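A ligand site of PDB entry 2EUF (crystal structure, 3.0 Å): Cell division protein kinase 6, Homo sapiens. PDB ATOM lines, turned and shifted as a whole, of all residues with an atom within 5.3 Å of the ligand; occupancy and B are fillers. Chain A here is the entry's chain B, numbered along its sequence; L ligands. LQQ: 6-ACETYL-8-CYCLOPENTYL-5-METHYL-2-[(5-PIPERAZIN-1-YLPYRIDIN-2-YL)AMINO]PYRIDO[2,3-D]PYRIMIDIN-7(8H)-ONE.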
ATOM      1  N   ILE A  19     -20.606  17.124  19.077  1.00  0.00           N
ATOM      2  CA  ILE A  19     -20.716  18.567  19.304  1.00  0.00           C
ATOM      3  C   ILE A  19     -19.642  19.427  18.588  1.00  0.00           C
ATOM      4  O   ILE A  19     -19.177  20.431  19.141  1.00  0.00           O
ATOM      5  CB  ILE A  19     -20.758  18.898  20.821  1.00  0.00           C
ATOM      6  CG1 ILE A  19     -19.732  18.051  21.580  1.00  0.00           C
ATOM      7  CG2 ILE A  19     -22.146  18.659  21.380  1.00  0.00           C
ATOM      8  CD1 ILE A  19     -19.291  18.656  22.894  1.00  0.00           C
ATOM      9  N   GLY A  20     -19.259  19.022  17.376  1.00  0.00           N
ATOM     10  CA  GLY A  20     -18.410  19.859  16.507  1.00  0.00           C
ATOM     11  C   GLY A  20     -17.004  19.389  16.174  1.00  0.00           C
ATOM     12  O   GLY A  20     -16.307  18.841  17.030  1.00  0.00           O
ATOM     13  N   GLU A  21     -16.593  19.645  14.930  1.00  0.00           N
ATOM     14  CA  GLU A  21     -15.279  19.254  14.426  1.00  0.00           C
ATOM     15  C   GLU A  21     -14.188  20.268  14.819  1.00  0.00           C
ATOM     16  O   GLU A  21     -14.048  21.319  14.179  1.00  0.00           O
ATOM     17  CB  GLU A  21     -15.322  19.054  12.910  1.00  0.00           C
ATOM     18  N   GLY A  22     -13.421  19.921  15.862  1.00  0.00           N
ATOM     19  CA  GLY A  22     -12.460  20.827  16.491  1.00  0.00           C
ATOM     20  C   GLY A  22     -11.149  20.930  15.748  1.00  0.00           C
ATOM     21  O   GLY A  22     -11.104  20.731  14.526  1.00  0.00           O
ATOM     22  N   VAL A  27     -15.084  16.527  17.987  1.00  0.00           N
ATOM     23  CA  VAL A  27     -15.346  16.493  19.428  1.00  0.00           C
ATOM     24  C   VAL A  27     -16.757  15.908  19.699  1.00  0.00           C
ATOM     25  O   VAL A  27     -17.755  16.434  19.177  1.00  0.00           O
ATOM     26  CB  VAL A  27     -15.205  17.909  20.083  1.00  0.00           C
ATOM     27  CG1 VAL A  27     -15.540  17.868  21.571  1.00  0.00           C
ATOM     28  CG2 VAL A  27     -13.815  18.475  19.859  1.00  0.00           C
ATOM     29  N   ALA A  41     -16.457  15.779  27.635  1.00  0.00           N
ATOM     30  CA  ALA A  41     -16.193  16.233  26.253  1.00  0.00           C
ATOM     31  C   ALA A  41     -14.973  15.522  25.656  1.00  0.00           C
ATOM     32  O   ALA A  41     -13.846  15.702  26.130  1.00  0.00           O
ATOM     33  CB  ALA A  41     -15.999  17.757  26.220  1.00  0.00           C
ATOM     34  N   LYS A  43     -12.367  14.798  22.627  1.00  0.00           N
ATOM     35  CA  LYS A  43     -11.682  15.220  21.406  1.00  0.00           C
ATOM     36  C   LYS A  43     -10.894  14.042  20.839  1.00  0.00           C
ATOM     37  O   LYS A  43      -9.960  13.546  21.463  1.00  0.00           O
ATOM     38  CB  LYS A  43     -10.750  16.411  21.691  1.00  0.00           C
ATOM     39  CG  LYS A  43     -10.250  17.178  20.470  1.00  0.00           C
ATOM     40  CD  LYS A  43      -9.831  18.592  20.880  1.00  0.00           C
ATOM     41  CE  LYS A  43      -9.136  19.362  19.726  1.00  0.00           C
ATOM     42  NZ  LYS A  43      -8.732  20.771  20.087  1.00  0.00           N
ATOM     43  N   GLU A  61      -1.708  22.994  23.065  1.00  0.00           N
ATOM     44  CA  GLU A  61      -3.020  23.245  23.676  1.00  0.00           C
ATOM     45  C   GLU A  61      -3.205  22.580  25.050  1.00  0.00           C
ATOM     46  O   GLU A  61      -3.765  23.192  25.972  1.00  0.00           O
ATOM     47  CB  GLU A  61      -4.118  22.792  22.715  1.00  0.00           C
ATOM     48  CG  GLU A  61      -5.514  22.738  23.280  1.00  0.00           C
ATOM     49  CD  GLU A  61      -6.470  21.903  22.422  1.00  0.00           C
ATOM     50  OE1 GLU A  61      -5.988  21.008  21.692  1.00  0.00           O
ATOM     51  OE2 GLU A  61      -7.704  22.141  22.494  1.00  0.00           O
ATOM     52  N   VAL A  77     -12.294  26.548  29.947  1.00  0.00           N
ATOM     53  CA  VAL A  77     -12.642  25.143  29.899  1.00  0.00           C
ATOM     54  C   VAL A  77     -11.628  24.340  30.727  1.00  0.00           C
ATOM     55  O   VAL A  77     -10.524  24.837  30.987  1.00  0.00           O
ATOM     56  CB  VAL A  77     -12.826  24.659  28.432  1.00  0.00           C
ATOM     57  CG1 VAL A  77     -11.501  24.462  27.747  1.00  0.00           C
ATOM     58  CG2 VAL A  77     -13.667  23.413  28.382  1.00  0.00           C
ATOM     59  N   PHE A  98     -12.468  16.545  28.258  1.00  0.00           N
ATOM     60  CA  PHE A  98     -12.705  17.824  28.910  1.00  0.00           C
ATOM     61  C   PHE A  98     -14.046  17.843  29.612  1.00  0.00           C
ATOM     62  O   PHE A  98     -14.867  16.949  29.438  1.00  0.00           O
ATOM     63  CB  PHE A  98     -12.734  18.952  27.874  1.00  0.00           C
ATOM     64  CG  PHE A  98     -11.476  19.088  27.075  1.00  0.00           C
ATOM     65  CD1 PHE A  98     -11.350  18.448  25.850  1.00  0.00           C
ATOM     66  CD2 PHE A  98     -10.434  19.879  27.538  1.00  0.00           C
ATOM     67  CE1 PHE A  98     -10.189  18.579  25.099  1.00  0.00           C
ATOM     68  CE2 PHE A  98      -9.268  20.014  26.799  1.00  0.00           C
ATOM     69  CZ  PHE A  98      -9.143  19.366  25.586  1.00  0.00           C
ATOM     70  N   GLU A  99     -14.281  18.898  30.387  1.00  0.00           N
ATOM     71  CA  GLU A  99     -15.617  19.152  30.902  1.00  0.00           C
ATOM     72  C   GLU A  99     -16.569  19.444  29.734  1.00  0.00           C
ATOM     73  O   GLU A  99     -16.202  20.154  28.788  1.00  0.00           O
ATOM     74  CB  GLU A  99     -15.622  20.252  31.972  1.00  0.00           C
ATOM     75  CG  GLU A  99     -15.337  21.681  31.496  1.00  0.00           C
ATOM     76  CD  GLU A  99     -15.578  22.744  32.560  1.00  0.00           C
ATOM     77  OE1 GLU A  99     -16.455  22.577  33.439  1.00  0.00           O
ATOM     78  OE2 GLU A  99     -14.886  23.773  32.533  1.00  0.00           O
ATOM     79  N   HIS A 100     -17.762  18.857  29.768  1.00  0.00           N
ATOM     80  CA  HIS A 100     -18.786  19.138  28.777  1.00  0.00           C
ATOM     81  C   HIS A 100     -19.533  20.427  29.126  1.00  0.00           C
ATOM     82  O   HIS A 100     -19.774  20.704  30.307  1.00  0.00           O
ATOM     83  CB  HIS A 100     -19.756  17.973  28.626  1.00  0.00           C
ATOM     84  CG  HIS A 100     -20.928  18.287  27.746  1.00  0.00           C
ATOM     85  ND1 HIS A 100     -22.218  18.388  28.236  1.00  0.00           N
ATOM     86  CD2 HIS A 100     -20.998  18.558  26.426  1.00  0.00           C
ATOM     87  CE1 HIS A 100     -23.036  18.682  27.240  1.00  0.00           C
ATOM     88  NE2 HIS A 100     -22.327  18.797  26.124  1.00  0.00           N
ATOM     89  N   VAL A 101     -19.867  21.213  28.120  1.00  0.00           N
ATOM     90  CA  VAL A 101     -20.636  22.433  28.302  1.00  0.00           C
ATOM     91  C   VAL A 101     -21.810  22.358  27.350  1.00  0.00           C
ATOM     92  O   VAL A 101     -21.706  21.815  26.250  1.00  0.00           O
ATOM     93  CB  VAL A 101     -19.762  23.720  28.180  1.00  0.00           C
ATOM     94  CG1 VAL A 101     -20.603  24.973  28.040  1.00  0.00           C
ATOM     95  CG2 VAL A 101     -18.869  23.873  29.381  1.00  0.00           C
ATOM     96  N   ASP A 102     -22.940  22.904  27.788  1.00  0.00           N
ATOM     97  CA  ASP A 102     -24.247  22.589  27.219  1.00  0.00           C
ATOM     98  C   ASP A 102     -24.421  22.974  25.753  1.00  0.00           C
ATOM     99  O   ASP A 102     -25.009  22.220  24.961  1.00  0.00           O
ATOM    100  CB  ASP A 102     -25.330  23.247  28.079  1.00  0.00           C
ATOM    101  CG  ASP A 102     -26.724  22.844  27.665  1.00  0.00           C
ATOM    102  OD1 ASP A 102     -26.958  21.631  27.445  1.00  0.00           O
ATOM    103  OD2 ASP A 102     -27.650  23.665  27.551  1.00  0.00           O
ATOM    104  N   GLN A 103     -23.914  24.147  25.414  1.00  0.00           N
ATOM    105  CA  GLN A 103     -24.051  24.696  24.081  1.00  0.00           C
ATOM    106  C   GLN A 103     -22.940  25.705  23.922  1.00  0.00           C
ATOM    107  O   GLN A 103     -22.241  26.014  24.884  1.00  0.00           O
ATOM    108  CB  GLN A 103     -25.402  25.378  23.936  1.00  0.00           C
ATOM    109  CG  GLN A 103     -25.651  26.453  24.975  1.00  0.00           C
ATOM    110  CD  GLN A 103     -26.886  27.284  24.705  1.00  0.00           C
ATOM    111  OE1 GLN A 103     -27.612  27.056  23.715  1.00  0.00           O
ATOM    112  NE2 GLN A 103     -27.152  28.259  25.570  1.00  0.00           N
ATOM    113  N   ASP A 104     -22.781  26.208  22.700  1.00  0.00           N
ATOM    114  CA  ASP A 104     -21.825  27.272  22.420  1.00  0.00           C
ATOM    115  C   ASP A 104     -22.575  28.596  22.291  1.00  0.00           C
ATOM    116  O   ASP A 104     -23.799  28.601  22.381  1.00  0.00           O
ATOM    117  CB  ASP A 104     -21.032  26.967  21.139  1.00  0.00           C
ATOM    118  CG  ASP A 104     -21.898  26.999  19.882  1.00  0.00           C
ATOM    119  OD1 ASP A 104     -23.146  27.019  19.984  1.00  0.00           O
ATOM    120  OD2 ASP A 104     -21.398  27.006  18.744  1.00  0.00           O
ATOM    121  N   THR A 106     -22.861  30.287  19.505  1.00  0.00           N
ATOM    122  CA  THR A 106     -23.578  30.182  18.209  1.00  0.00           C
ATOM    123  C   THR A 106     -24.992  29.651  18.388  1.00  0.00           C
ATOM    124  O   THR A 106     -25.953  30.389  18.159  1.00  0.00           O
ATOM    125  CB  THR A 106     -22.770  29.328  17.143  1.00  0.00           C
ATOM    126  OG1 THR A 106     -21.967  30.179  16.319  1.00  0.00           O
ATOM    127  CG2 THR A 106     -23.699  28.673  16.111  1.00  0.00           C
ATOM    128  N   THR A 107     -25.101  28.387  18.806  1.00  0.00           N
ATOM    129  CA  THR A 107     -26.380  27.693  19.050  1.00  0.00           C
ATOM    130  C   THR A 107     -27.275  28.485  19.988  1.00  0.00           C
ATOM    131  O   THR A 107     -28.481  28.554  19.790  1.00  0.00           O
ATOM    132  CB  THR A 107     -26.114  26.266  19.608  1.00  0.00           C
ATOM    133  OG1 THR A 107     -25.539  25.452  18.586  1.00  0.00           O
ATOM    134  CG2 THR A 107     -27.413  25.541  19.943  1.00  0.00           C
ATOM    135  N   GLN A 149     -18.228  30.034  18.112  1.00  0.00           N
ATOM    136  CA  GLN A 149     -18.183  28.575  18.269  1.00  0.00           C
ATOM    137  C   GLN A 149     -17.232  28.077  19.353  1.00  0.00           C
ATOM    138  O   GLN A 149     -17.389  26.968  19.860  1.00  0.00           O
ATOM    139  CB  GLN A 149     -17.853  27.927  16.944  1.00  0.00           C
ATOM    140  CG  GLN A 149     -18.942  28.150  15.952  1.00  0.00           C
ATOM    141  CD  GLN A 149     -18.424  28.733  14.664  1.00  0.00           C
ATOM    142  OE1 GLN A 149     -17.379  28.302  14.151  1.00  0.00           O
ATOM    143  NE2 GLN A 149     -19.168  29.695  14.129  1.00  0.00           N
ATOM    144  N   ASN A 150     -16.239  28.898  19.688  1.00  0.00           N
ATOM    145  CA  ASN A 150     -15.282  28.561  20.742  1.00  0.00           C
ATOM    146  C   ASN A 150     -15.725  29.089  22.116  1.00  0.00           C
ATOM    147  O   ASN A 150     -15.223  28.646  23.146  1.00  0.00           O
ATOM    148  CB  ASN A 150     -13.869  29.062  20.381  1.00  0.00           C
ATOM    149  CG  ASN A 150     -13.204  28.255  19.233  1.00  0.00           C
ATOM    150  OD1 ASN A 150     -13.660  27.163  18.862  1.00  0.00           O
ATOM    151  ND2 ASN A 150     -12.129  28.803  18.689  1.00  0.00           N
ATOM    152  N   LEU A 152     -18.200  29.104  25.030  1.00  0.00           N
ATOM    153  CA  LEU A 152     -19.171  28.153  25.555  1.00  0.00           C
ATOM    154  C   LEU A 152     -20.013  28.734  26.680  1.00  0.00           C
ATOM    155  O   LEU A 152     -19.499  29.433  27.552  1.00  0.00           O
ATOM    156  CB  LEU A 152     -18.472  26.878  26.039  1.00  0.00           C
ATOM    157  CG  LEU A 152     -17.522  26.189  25.073  1.00  0.00           C
ATOM    158  CD1 LEU A 152     -17.061  24.923  25.720  1.00  0.00           C
ATOM    159  CD2 LEU A 152     -18.192  25.895  23.733  1.00  0.00           C
ATOM    160  N   ALA A 162     -13.060  28.028  24.823  1.00  0.00           N
ATOM    161  CA  ALA A 162     -12.691  26.674  24.445  1.00  0.00           C
ATOM    162  C   ALA A 162     -11.745  26.637  23.262  1.00  0.00           C
ATOM    163  O   ALA A 162     -11.311  27.674  22.785  1.00  0.00           O
ATOM    164  CB  ALA A 162     -13.901  25.839  24.176  1.00  0.00           C
ATOM    165  N   ASP A 163     -11.428  25.417  22.789  1.00  0.00           N
ATOM    166  CA  ASP A 163     -10.409  25.170  21.768  1.00  0.00           C
ATOM    167  C   ASP A 163      -9.175  26.058  21.936  1.00  0.00           C
ATOM    168  O   ASP A 163      -9.135  27.160  21.404  1.00  0.00           O
ATOM    169  CB  ASP A 163     -10.983  25.301  20.352  1.00  0.00           C
ATOM    170  CG  ASP A 163     -10.008  24.786  19.288  1.00  0.00           C
ATOM    171  OD1 ASP A 163      -8.767  24.959  19.430  1.00  0.00           O
ATOM    172  OD2 ASP A 163     -10.402  24.176  18.263  1.00  0.00           O
ATOM    173  N   PHE A 164      -8.189  25.549  22.657  1.00  0.00           N
ATOM    174  CA  PHE A 164      -6.927  26.276  22.889  1.00  0.00           C
ATOM    175  C   PHE A 164      -5.795  25.849  21.947  1.00  0.00           C
ATOM    176  O   PHE A 164      -4.618  26.081  22.221  1.00  0.00           O
ATOM    177  CB  PHE A 164      -6.483  26.146  24.340  1.00  0.00           C
ATOM    178  CG  PHE A 164      -7.171  27.102  25.264  1.00  0.00           C
ATOM    179  CD1 PHE A 164      -6.543  28.278  25.665  1.00  0.00           C
ATOM    180  CD2 PHE A 164      -8.462  26.852  25.701  1.00  0.00           C
ATOM    181  CE1 PHE A 164      -7.176  29.175  26.518  1.00  0.00           C
ATOM    182  CE2 PHE A 164      -9.103  27.744  26.550  1.00  0.00           C
ATOM    183  CZ  PHE A 164      -8.457  28.905  26.949  1.00  0.00           C
HETATM  184  O01 LQQ L   1     -11.824  23.115  24.164  1.00  0.00           O
HETATM  185  C02 LQQ L   1     -12.397  22.142  23.739  1.00  0.00           C
HETATM  186  C01 LQQ L   1     -11.670  20.905  23.314  1.00  0.00           C
HETATM  187  C03 LQQ L   1     -13.894  22.179  23.610  1.00  0.00           C
HETATM  188  C04 LQQ L   1     -14.735  21.837  24.677  1.00  0.00           C
HETATM  189  C05 LQQ L   1     -14.214  21.488  26.043  1.00  0.00           C
HETATM  190  C06 LQQ L   1     -16.186  22.022  24.492  1.00  0.00           C
HETATM  191  C07 LQQ L   1     -17.147  21.579  25.507  1.00  0.00           C
HETATM  192  N01 LQQ L   1     -18.450  21.688  25.267  1.00  0.00           N
HETATM  193  C08 LQQ L   1     -18.925  22.023  24.050  1.00  0.00           C
HETATM  194  N02 LQQ L   1     -18.062  22.315  23.017  1.00  0.00           N
HETATM  195  C09 LQQ L   1     -16.706  22.247  23.156  1.00  0.00           C
HETATM  196  N03 LQQ L   1     -15.847  22.576  22.152  1.00  0.00           N
HETATM  197  C10 LQQ L   1     -16.391  22.916  20.831  1.00  0.00           C
HETATM  198  C11 LQQ L   1     -15.831  24.185  20.195  1.00  0.00           C
HETATM  199  C12 LQQ L   1     -15.596  23.861  18.713  1.00  0.00           C
HETATM  200  C13 LQQ L   1     -15.866  22.367  18.476  1.00  0.00           C
HETATM  201  C14 LQQ L   1     -16.116  21.764  19.851  1.00  0.00           C
HETATM  202  C15 LQQ L   1     -14.434  22.525  22.366  1.00  0.00           C
HETATM  203  O02 LQQ L   1     -13.618  22.789  21.435  1.00  0.00           O
HETATM  204  N04 LQQ L   1     -20.283  22.042  23.946  1.00  0.00           N
HETATM  205  C16 LQQ L   1     -21.041  22.248  22.839  1.00  0.00           C
HETATM  206  N05 LQQ L   1     -22.352  21.925  22.885  1.00  0.00           N
HETATM  207  C17 LQQ L   1     -23.155  22.112  21.827  1.00  0.00           C
HETATM  208  C18 LQQ L   1     -22.651  22.661  20.654  1.00  0.00           C
HETATM  209  C19 LQQ L   1     -21.311  23.012  20.586  1.00  0.00           C
HETATM  210  C20 LQQ L   1     -20.500  22.803  21.681  1.00  0.00           C
HETATM  211  N06 LQQ L   1     -23.493  22.862  19.525  1.00  0.00           N
HETATM  212  C21 LQQ L   1     -24.064  21.560  19.101  1.00  0.00           C
HETATM  213  C22 LQQ L   1     -25.026  21.759  17.924  1.00  0.00           C
HETATM  214  N07 LQQ L   1     -24.374  22.507  16.851  1.00  0.00           N
HETATM  215  C23 LQQ L   1     -23.531  23.664  17.135  1.00  0.00           C
HETATM  216  C24 LQQ L   1     -22.739  23.550  18.444  1.00  0.00           C
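A nitrogen (N04) of the ligand lies close to the backbone carbonyl oxygen of Val 101 (2.7 Å). The backbone NH (N) of Asp 163 lies within hydrogen-bond range of an oxygen (O01) of the ligand (2.7 Å). N of Val 101 is in hydrogen-bond range of N01 of the ligand, at 3.2 Å.
OD1 of Asp 104 lies close to N of Thr 106 (3.3 Å). The backbone NH (N) of Phe 98 sits at hydrogen-bond distance from the backbone carbonyl oxygen (O) of Ala 41 (2.7 Å). The backbone carbonyl oxygen of Val 27 is in hydrogen-bond range of the backbone NH of Ile 19 (2.9 Å). The backbone carbonyl oxygen (O) of Asn 150 is in hydrogen-bond range of the backbone NH (N) of Ala 162 (2.8 Å). The side-chain amino group (NZ) of Lys 43 lies within salt-bridge range of the side-chain carboxylate (OE2) of Glu 61, 3.0 Å away. The backbone carbonyl oxygen of Gly 20 lies within hydrogen-bond range of the backbone NH of Val 27 (2.8 Å). N of Thr 107 sits at hydrogen-bond distance from OD1 of Asp 104 (2.7 Å).
A nitrogen (N05) of the ligand sits close to the backbone carbonyl oxygen (O) of Asp 102 (3.4 Å). OG1 of Thr 107 sits close to N06 of the ligand (3.4 Å). O of Ile 19 touches C14 of the ligand (3.4 Å). Gly 20 touches the ligand (O to C13, 3.8 Å). CB of Val 27 touches C14 of the ligand (3.97 Å). Lys 43 touches the ligand (CD to C01, 3.8 Å). CG2 of Val 77 touches C05 of the ligand, 3.1 Å away. Phe 98 touches the ligand. Glu 99 touches the ligand (O to C05, 3.6 Å). Gln 103 touches the ligand. OD2 of Asp 104 touches C24 of the ligand, at 3.7 Å. Gln 149 touches the ligand. Asn 150 touches the ligand (OD1 to C12, 3.8 Å). CD1 of Leu 152 touches C06 of the ligand (3.3 Å). Ala 162 touches the ligand (CB to O01, 3.4 Å). Within 4 Å of the ligand: Ile 19, Gly 20, Val 27, Lys 43, Val 77, Phe 98, Glu 99, Val 101, Asp 102, Gln 103, Asp 104, Thr 107, Gln 149, Asn 150, Leu 152, Ala 162 and Asp 163. The nearest printed residue that does not touch the ligand is Ala 41 (4.1 Å).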
